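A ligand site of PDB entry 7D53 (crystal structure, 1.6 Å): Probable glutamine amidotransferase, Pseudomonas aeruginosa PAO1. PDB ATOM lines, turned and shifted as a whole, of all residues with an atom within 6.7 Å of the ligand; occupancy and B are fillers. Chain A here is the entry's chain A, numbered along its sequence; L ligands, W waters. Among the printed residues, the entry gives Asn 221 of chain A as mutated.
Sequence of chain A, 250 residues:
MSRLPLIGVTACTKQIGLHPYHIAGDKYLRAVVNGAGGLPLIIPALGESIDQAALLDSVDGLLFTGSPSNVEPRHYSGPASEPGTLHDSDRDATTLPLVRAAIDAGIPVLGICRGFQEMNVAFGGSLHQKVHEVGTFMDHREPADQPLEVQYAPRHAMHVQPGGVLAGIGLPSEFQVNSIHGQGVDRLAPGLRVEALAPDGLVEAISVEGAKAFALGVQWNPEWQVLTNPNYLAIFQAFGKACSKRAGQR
OD1 of Asn 70 sits at hydrogen-bond distance from N1 of the ligand, at 2.7 Å. N1 of the ligand lies within hydrogen-bond range of O of Ser 69, at 2.9 Å. N of Ser 67 sits at hydrogen-bond distance from O2 of the ligand, 2.9 Å away. The backbone carbonyl oxygen (O) of Ser 67 sits close to a nitrogen (N1) of the ligand, at 3.4 Å. O4 of the ligand sits at hydrogen-bond distance from N of Gly 182 (2.9 Å). O1 of the ligand lies within hydrogen-bond range of NE2 of Gln 117 (2.9 Å). N of Gln 183 lies within hydrogen-bond range of O1 of the ligand (3.0 Å). SG of Cys 113 sits close to O2 of the ligand (3.0 Å). O2 of the ligand is in hydrogen-bond range of N of Arg 114 (3.0 Å). N1 of the ligand lies within hydrogen-bond range of O of Pro 68 (3.2 Å).
The side-chain amide oxygen of Asn 70 lies close to the side-chain amide nitrogen of Gln 183, at 3.3 Å. The backbone carbonyl oxygen (O) of Asn 70 is in hydrogen-bond range of the guanidinium group (NH2) of Arg 114, at 3.3 Å. N of Asn 70 lies within hydrogen-bond range of O of Leu 86 (2.9 Å). The backbone NH (N) of Ser 69 is in hydrogen-bond range of the side-chain hydroxyl (OG) of Ser 67, 3.1 Å away. ND1 of His 181 lies within hydrogen-bond range of O of Gln 183. The side-chain sulfur (SG) of Cys 113 lies close to the side-chain amide oxygen (OD1) of Asn 221, 3.7 Å away. O of Ile 112 sits at hydrogen-bond distance from N of Gly 66 (3.2 Å). O of His 181 is in hydrogen-bond range of N of Arg 141.
Residues that only touch the ligand: Gly 66 (3.2 Å), Ile 180 (3.5 Å) and His 181 (3.3 Å). Hydrophobic or aromatic side chains within 4 Å of the ligand: His 181. 12 residues have an atom within 4 Å of the ligand: Gly 66, Ser 67, Pro 68, Ser 69, Asn 70, Cys 113, Arg 114, Gln 117, Ile 180, His 181, Gly 182 and Gln 183. The nearest printed residue that does not touch the ligand is Asn 221 (4.7 Å).
Water W2 bridges an oxygen (O4) of the ligand (2.8 Å) and the side-chain amide oxygen (OD1) of Asn 70 (3.5 Å). Water W1 bridges N1 of the ligand (3.1 Å) and O of Pro 68 (3.4 Å).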
ATOM      1  N   TYR A  28     -13.698 -34.202  -7.571  1.00  0.00           N
ATOM      2  CA  TYR A  28     -12.340 -33.687  -7.510  1.00  0.00           C
ATOM      3  C   TYR A  28     -11.324 -34.814  -7.620  1.00  0.00           C
ATOM      4  O   TYR A  28     -10.282 -34.687  -8.295  1.00  0.00           O
ATOM      5  CB  TYR A  28     -12.103 -32.923  -6.200  1.00  0.00           C
ATOM      6  CG  TYR A  28     -12.926 -31.687  -6.068  1.00  0.00           C
ATOM      7  CD1 TYR A  28     -12.587 -30.537  -6.780  1.00  0.00           C
ATOM      8  CD2 TYR A  28     -14.046 -31.655  -5.241  1.00  0.00           C
ATOM      9  CE1 TYR A  28     -13.350 -29.388  -6.708  1.00  0.00           C
ATOM     10  CE2 TYR A  28     -14.820 -30.489  -5.122  1.00  0.00           C
ATOM     11  CZ  TYR A  28     -14.465 -29.377  -5.869  1.00  0.00           C
ATOM     12  OH  TYR A  28     -15.191 -28.199  -5.792  1.00  0.00           O
ATOM     13  N   THR A  65      -9.739 -27.929  -2.759  1.00  0.00           N
ATOM     14  CA  THR A  65     -11.003 -28.155  -3.427  1.00  0.00           C
ATOM     15  C   THR A  65     -12.005 -27.034  -3.157  1.00  0.00           C
ATOM     16  O   THR A  65     -11.853 -26.224  -2.242  1.00  0.00           O
ATOM     17  CB  THR A  65     -11.661 -29.428  -2.923  1.00  0.00           C
ATOM     18  OG1 THR A  65     -11.782 -29.321  -1.517  1.00  0.00           O
ATOM     19  CG2 THR A  65     -10.814 -30.632  -3.225  1.00  0.00           C
ATOM     20  N   GLY A  66     -13.065 -27.011  -3.966  1.00  0.00           N
ATOM     21  CA  GLY A  66     -14.251 -26.228  -3.624  1.00  0.00           C
ATOM     22  C   GLY A  66     -15.051 -26.841  -2.500  1.00  0.00           C
ATOM     23  O   GLY A  66     -14.857 -27.983  -2.093  1.00  0.00           O
ATOM     24  N   SER A  67     -15.958 -26.043  -1.949  1.00  0.00           N
ATOM     25  CA  SER A  67     -16.826 -26.487  -0.860  1.00  0.00           C
ATOM     26  C   SER A  67     -17.989 -25.540  -0.734  1.00  0.00           C
ATOM     27  O   SER A  67     -17.858 -24.365  -1.068  1.00  0.00           O
ATOM     28  CB  SER A  67     -16.049 -26.541   0.469  1.00  0.00           C
ATOM     29  OG  SER A  67     -16.938 -26.836   1.544  1.00  0.00           O
ATOM     30  N   PRO A  68     -19.148 -26.003  -0.244  1.00  0.00           N
ATOM     31  CA  PRO A  68     -20.207 -25.043   0.088  1.00  0.00           C
ATOM     32  C   PRO A  68     -19.837 -24.103   1.217  1.00  0.00           C
ATOM     33  O   PRO A  68     -20.468 -23.045   1.343  1.00  0.00           O
ATOM     34  CB  PRO A  68     -21.399 -25.946   0.490  1.00  0.00           C
ATOM     35  CG  PRO A  68     -20.836 -27.320   0.661  1.00  0.00           C
ATOM     36  CD  PRO A  68     -19.577 -27.412  -0.139  1.00  0.00           C
ATOM     37  N   SER A  69     -18.847 -24.438   2.041  1.00  0.00           N
ATOM     38  CA  SER A  69     -18.510 -23.565   3.166  1.00  0.00           C
ATOM     39  C   SER A  69     -17.703 -22.365   2.670  1.00  0.00           C
ATOM     40  O   SER A  69     -17.192 -22.354   1.571  1.00  0.00           O
ATOM     41  CB  SER A  69     -17.725 -24.313   4.239  1.00  0.00           C
ATOM     42  OG  SER A  69     -16.408 -24.574   3.768  1.00  0.00           O
ATOM     43  N   ASN A  70     -17.552 -21.373   3.537  1.00  0.00           N
ATOM     44  CA  ASN A  70     -16.896 -20.107   3.250  1.00  0.00           C
ATOM     45  C   ASN A  70     -15.810 -19.871   4.280  1.00  0.00           C
ATOM     46  O   ASN A  70     -15.982 -20.207   5.467  1.00  0.00           O
ATOM     47  CB  ASN A  70     -17.914 -18.959   3.313  1.00  0.00           C
ATOM     48  CG  ASN A  70     -19.094 -19.200   2.393  1.00  0.00           C
ATOM     49  OD1 ASN A  70     -19.002 -19.016   1.206  1.00  0.00           O
ATOM     50  ND2 ASN A  70     -20.209 -19.668   2.951  1.00  0.00           N
ATOM     51  N   VAL A  71     -14.672 -19.340   3.819  1.00  0.00           N
ATOM     52  CA  VAL A  71     -13.609 -18.956   4.749  1.00  0.00           C
ATOM     53  C   VAL A  71     -14.173 -17.981   5.773  1.00  0.00           C
ATOM     54  O   VAL A  71     -14.888 -17.021   5.430  1.00  0.00           O
ATOM     55  CB  VAL A  71     -12.448 -18.298   3.986  1.00  0.00           C
ATOM     56  CG1 VAL A  71     -11.345 -17.843   4.949  1.00  0.00           C
ATOM     57  CG2 VAL A  71     -11.895 -19.241   2.919  1.00  0.00           C
ATOM     58  N   LEU A  86     -22.447 -20.780   6.059  1.00  0.00           N
ATOM     59  CA  LEU A  86     -21.745 -22.024   6.302  1.00  0.00           C
ATOM     60  C   LEU A  86     -20.249 -21.785   6.415  1.00  0.00           C
ATOM     61  O   LEU A  86     -19.656 -21.170   5.529  1.00  0.00           O
ATOM     62  CB  LEU A  86     -22.032 -23.011   5.173  1.00  0.00           C
ATOM     63  CG  LEU A  86     -23.508 -23.328   4.924  1.00  0.00           C
ATOM     64  CD1 LEU A  86     -23.750 -23.974   3.571  1.00  0.00           C
ATOM     65  CD2 LEU A  86     -24.015 -24.227   6.055  1.00  0.00           C
ATOM     66  N   ILE A 112      -9.184 -24.529  -6.406  1.00  0.00           N
ATOM     67  CA  ILE A 112     -10.457 -24.448  -7.125  1.00  0.00           C
ATOM     68  C   ILE A 112     -11.516 -23.829  -6.212  1.00  0.00           C
ATOM     69  O   ILE A 112     -11.794 -24.351  -5.128  1.00  0.00           O
ATOM     70  CB  ILE A 112     -10.908 -25.847  -7.599  1.00  0.00           C
ATOM     71  CG1 ILE A 112      -9.981 -26.347  -8.708  1.00  0.00           C
ATOM     72  CG2 ILE A 112     -12.353 -25.763  -8.120  1.00  0.00           C
ATOM     73  CD1 ILE A 112     -10.253 -27.744  -9.127  1.00  0.00           C
ATOM     74  N   CYS A 113     -12.157 -22.760  -6.686  1.00  0.00           N
ATOM     75  CA  CYS A 113     -13.322 -22.103  -6.069  1.00  0.00           C
ATOM     76  C   CYS A 113     -13.022 -21.745  -4.616  1.00  0.00           C
ATOM     77  O   CYS A 113     -12.234 -20.820  -4.415  1.00  0.00           O
ATOM     78  CB  CYS A 113     -14.573 -22.984  -6.258  1.00  0.00           C
ATOM     79  SG  CYS A 113     -16.116 -21.995  -6.042  1.00  0.00           S
ATOM     80  N   ARG A 114     -13.587 -22.420  -3.616  1.00  0.00           N
ATOM     81  CA  ARG A 114     -13.197 -22.116  -2.241  1.00  0.00           C
ATOM     82  C   ARG A 114     -11.687 -22.144  -2.050  1.00  0.00           C
ATOM     83  O   ARG A 114     -11.105 -21.322  -1.325  1.00  0.00           O
ATOM     84  CB  ARG A 114     -13.838 -23.089  -1.243  1.00  0.00           C
ATOM     85  CG  ARG A 114     -13.676 -22.601   0.206  1.00  0.00           C
ATOM     86  CD  ARG A 114     -13.337 -23.707   1.178  1.00  0.00           C
ATOM     87  NE  ARG A 114     -14.041 -23.510   2.450  1.00  0.00           N
ATOM     88  CZ  ARG A 114     -13.473 -23.092   3.585  1.00  0.00           C
ATOM     89  NH1 ARG A 114     -12.174 -22.835   3.653  1.00  0.00           N
ATOM     90  NH2 ARG A 114     -14.236 -22.940   4.652  1.00  0.00           N
ATOM     91  N   GLY A 115     -11.004 -23.065  -2.738  1.00  0.00           N
ATOM     92  CA  GLY A 115      -9.568 -23.172  -2.580  1.00  0.00           C
ATOM     93  C   GLY A 115      -8.791 -22.020  -3.177  1.00  0.00           C
ATOM     94  O   GLY A 115      -7.747 -21.624  -2.640  1.00  0.00           O
ATOM     95  N   GLN A 117     -10.155 -19.007  -3.195  1.00  0.00           N
ATOM     96  CA  GLN A 117     -10.418 -17.974  -2.197  1.00  0.00           C
ATOM     97  C   GLN A 117      -9.472 -18.130  -1.011  1.00  0.00           C
ATOM     98  O   GLN A 117      -8.979 -17.124  -0.477  1.00  0.00           O
ATOM     99  CB  GLN A 117     -11.883 -18.074  -1.750  1.00  0.00           C
ATOM    100  CG  GLN A 117     -12.843 -17.733  -2.847  1.00  0.00           C
ATOM    101  CD  GLN A 117     -14.251 -18.176  -2.586  1.00  0.00           C
ATOM    102  OE1 GLN A 117     -14.556 -18.761  -1.564  1.00  0.00           O
ATOM    103  NE2 GLN A 117     -15.144 -17.832  -3.543  1.00  0.00           N
ATOM    104  N   HIS A 128     -15.133 -10.557  -1.024  1.00  0.00           N
ATOM    105  CA  HIS A 128     -16.505 -10.105  -0.966  1.00  0.00           C
ATOM    106  C   HIS A 128     -17.346 -11.270  -0.479  1.00  0.00           C
ATOM    107  O   HIS A 128     -17.304 -12.344  -1.073  1.00  0.00           O
ATOM    108  CB  HIS A 128     -17.026  -9.686  -2.329  1.00  0.00           C
ATOM    109  CG  HIS A 128     -16.380  -8.470  -2.925  1.00  0.00           C
ATOM    110  ND1 HIS A 128     -16.488  -7.219  -2.360  1.00  0.00           N
ATOM    111  CD2 HIS A 128     -15.635  -8.313  -4.042  1.00  0.00           C
ATOM    112  CE1 HIS A 128     -15.820  -6.347  -3.100  1.00  0.00           C
ATOM    113  NE2 HIS A 128     -15.303  -6.977  -4.133  1.00  0.00           N
ATOM    114  N   GLN A 129     -18.133 -11.095   0.561  1.00  0.00           N
ATOM    115  CA  GLN A 129     -18.913 -12.226   1.024  1.00  0.00           C
ATOM    116  C   GLN A 129     -20.154 -12.479   0.182  1.00  0.00           C
ATOM    117  O   GLN A 129     -20.696 -13.596   0.226  1.00  0.00           O
ATOM    118  CB  GLN A 129     -19.294 -12.053   2.502  1.00  0.00           C
ATOM    119  CG  GLN A 129     -18.077 -12.226   3.391  1.00  0.00           C
ATOM    120  CD  GLN A 129     -18.375 -12.060   4.847  1.00  0.00           C
ATOM    121  OE1 GLN A 129     -19.159 -12.818   5.429  1.00  0.00           O
ATOM    122  NE2 GLN A 129     -17.749 -11.070   5.450  1.00  0.00           N
ATOM    123  N   ARG A 141     -23.401 -17.010  -8.681  1.00  0.00           N
ATOM    124  CA  ARG A 141     -23.922 -18.247  -8.145  1.00  0.00           C
ATOM    125  C   ARG A 141     -24.542 -19.118  -9.209  1.00  0.00           C
ATOM    126  O   ARG A 141     -24.983 -18.656 -10.266  1.00  0.00           O
ATOM    127  CB  ARG A 141     -24.974 -17.937  -7.061  1.00  0.00           C
ATOM    128  CG  ARG A 141     -24.434 -17.106  -5.894  1.00  0.00           C
ATOM    129  CD  ARG A 141     -25.573 -16.677  -4.946  1.00  0.00           C
ATOM    130  NE  ARG A 141     -26.441 -15.787  -5.632  1.00  0.00           N
ATOM    131  CZ  ARG A 141     -27.536 -15.242  -5.112  1.00  0.00           C
ATOM    132  NH1 ARG A 141     -27.848 -15.521  -3.844  1.00  0.00           N
ATOM    133  NH2 ARG A 141     -28.298 -14.461  -5.837  1.00  0.00           N
ATOM    134  N   TYR A 152     -23.546 -26.569 -13.337  1.00  0.00           N
ATOM    135  CA  TYR A 152     -22.096 -26.589 -13.562  1.00  0.00           C
ATOM    136  C   TYR A 152     -21.703 -26.426 -15.027  1.00  0.00           C
ATOM    137  O   TYR A 152     -20.518 -26.557 -15.365  1.00  0.00           O
ATOM    138  CB  TYR A 152     -21.484 -27.889 -13.019  1.00  0.00           C
ATOM    139  CG  TYR A 152     -21.311 -27.907 -11.521  1.00  0.00           C
ATOM    140  CD1 TYR A 152     -22.396 -28.063 -10.678  1.00  0.00           C
ATOM    141  CD2 TYR A 152     -20.049 -27.739 -10.942  1.00  0.00           C
ATOM    142  CE1 TYR A 152     -22.236 -28.054  -9.301  1.00  0.00           C
ATOM    143  CE2 TYR A 152     -19.896 -27.726  -9.588  1.00  0.00           C
ATOM    144  CZ  TYR A 152     -20.991 -27.891  -8.766  1.00  0.00           C
ATOM    145  OH  TYR A 152     -20.871 -27.883  -7.398  1.00  0.00           O
ATOM    146  N   ILE A 180     -20.098 -21.103  -9.730  1.00  0.00           N
ATOM    147  CA  ILE A 180     -20.879 -21.682  -8.639  1.00  0.00           C
ATOM    148  C   ILE A 180     -20.407 -21.042  -7.348  1.00  0.00           C
ATOM    149  O   ILE A 180     -19.933 -21.734  -6.443  1.00  0.00           O
ATOM    150  CB  ILE A 180     -20.721 -23.214  -8.596  1.00  0.00           C
ATOM    151  CG1 ILE A 180     -20.977 -23.850  -9.995  1.00  0.00           C
ATOM    152  CG2 ILE A 180     -21.676 -23.834  -7.574  1.00  0.00           C
ATOM    153  CD1 ILE A 180     -19.714 -24.119 -10.756  1.00  0.00           C
ATOM    154  N   HIS A 181     -20.419 -19.713  -7.288  1.00  0.00           N
ATOM    155  CA  HIS A 181     -19.815 -19.083  -6.109  1.00  0.00           C
ATOM    156  C   HIS A 181     -20.539 -17.791  -5.743  1.00  0.00           C
ATOM    157  O   HIS A 181     -20.896 -16.990  -6.596  1.00  0.00           O
ATOM    158  CB  HIS A 181     -18.306 -18.784  -6.323  1.00  0.00           C
ATOM    159  CG  HIS A 181     -18.015 -17.915  -7.499  1.00  0.00           C
ATOM    160  ND1 HIS A 181     -17.590 -16.607  -7.340  1.00  0.00           N
ATOM    161  CD2 HIS A 181     -18.035 -18.145  -8.848  1.00  0.00           C
ATOM    162  CE1 HIS A 181     -17.401 -16.071  -8.534  1.00  0.00           C
ATOM    163  NE2 HIS A 181     -17.653 -16.978  -9.452  1.00  0.00           N
ATOM    164  N   GLY A 182     -20.786 -17.646  -4.439  1.00  0.00           N
ATOM    165  CA  GLY A 182     -21.344 -16.418  -3.907  1.00  0.00           C
ATOM    166  C   GLY A 182     -20.312 -15.438  -3.390  1.00  0.00           C
ATOM    167  O   GLY A 182     -20.623 -14.248  -3.259  1.00  0.00           O
ATOM    168  N   GLN A 183     -19.104 -15.909  -3.066  1.00  0.00           N
ATOM    169  CA  GLN A 183     -18.005 -15.062  -2.650  1.00  0.00           C
ATOM    170  C   GLN A 183     -16.983 -14.905  -3.778  1.00  0.00           C
ATOM    171  O   GLN A 183     -17.042 -15.599  -4.801  1.00  0.00           O
ATOM    172  CB  GLN A 183     -17.340 -15.637  -1.386  1.00  0.00           C
ATOM    173  CG  GLN A 183     -18.377 -15.991  -0.274  1.00  0.00           C
ATOM    174  CD  GLN A 183     -17.859 -15.971   1.132  1.00  0.00           C
ATOM    175  OE1 GLN A 183     -16.682 -16.155   1.387  1.00  0.00           O
ATOM    176  NE2 GLN A 183     -18.780 -15.791   2.083  1.00  0.00           N
ATOM    177  N   GLY A 184     -16.043 -13.990  -3.586  1.00  0.00           N
ATOM    178  CA  GLY A 184     -15.051 -13.713  -4.601  1.00  0.00           C
ATOM    179  C   GLY A 184     -14.017 -12.754  -4.037  1.00  0.00           C
ATOM    180  O   GLY A 184     -14.113 -12.281  -2.905  1.00  0.00           O
ATOM    181  N   GLN A 219     -11.338 -19.545  -9.844  1.00  0.00           N
ATOM    182  CA  GLN A 219     -12.606 -19.386  -9.136  1.00  0.00           C
ATOM    183  C   GLN A 219     -13.707 -20.274  -9.717  1.00  0.00           C
ATOM    184  O   GLN A 219     -14.696 -20.539  -9.014  1.00  0.00           O
ATOM    185  CB  GLN A 219     -13.014 -17.894  -9.203  1.00  0.00           C
ATOM    186  CG  GLN A 219     -14.348 -17.520  -8.559  1.00  0.00           C
ATOM    187  CD  GLN A 219     -14.348 -17.650  -7.067  1.00  0.00           C
ATOM    188  OE1 GLN A 219     -14.043 -16.716  -6.316  1.00  0.00           O
ATOM    189  NE2 GLN A 219     -14.705 -18.816  -6.605  1.00  0.00           N
ATOM    190  N   ASN A 221     -14.837 -24.046 -11.736  1.00  0.00           N
ATOM    191  CA  ASN A 221     -14.768 -25.425 -11.236  1.00  0.00           C
ATOM    192  C   ASN A 221     -14.354 -26.370 -12.348  1.00  0.00           C
ATOM    193  O   ASN A 221     -15.199 -27.051 -12.950  1.00  0.00           O
ATOM    194  CB  ASN A 221     -16.123 -25.847 -10.652  1.00  0.00           C
ATOM    195  CG  ASN A 221     -16.290 -25.414  -9.193  1.00  0.00           C
ATOM    196  OD1 ASN A 221     -16.591 -24.251  -8.905  1.00  0.00           O
ATOM    197  ND2 ASN A 221     -16.063 -26.331  -8.277  1.00  0.00           N
HETATM  198  N1  LIG L   1     -18.687 -21.079  -0.502  1.00  0.00           N
HETATM  199  C1  LIG L   1     -17.787 -20.432  -1.431  1.00  0.00           C
HETATM  200  C2  LIG L   1     -18.539 -19.411  -2.321  1.00  0.00           C
HETATM  201  O1  LIG L   1     -17.932 -18.619  -3.008  1.00  0.00           O
HETATM  202  C3  LIG L   1     -17.095 -21.472  -2.335  1.00  0.00           C
HETATM  203  C4  LIG L   1     -18.055 -22.148  -3.305  1.00  0.00           C
HETATM  204  C5  LIG L   1     -17.508 -23.449  -3.854  1.00  0.00           C
HETATM  205  O2  LIG L   1     -16.298 -23.750  -3.647  1.00  0.00           O
HETATM  206  O3  LIG L   1     -18.305 -24.171  -4.510  1.00  0.00           O
HETATM  207  O4  LIG L   1     -19.803 -19.373  -2.289  1.00  0.00           O
HETATM  208  O   HOH W   1     -21.252 -22.099  -1.819  1.00  0.00           O
HETATM  209  O   HOH W   2     -21.813 -18.222  -0.672  1.00  0.00           O
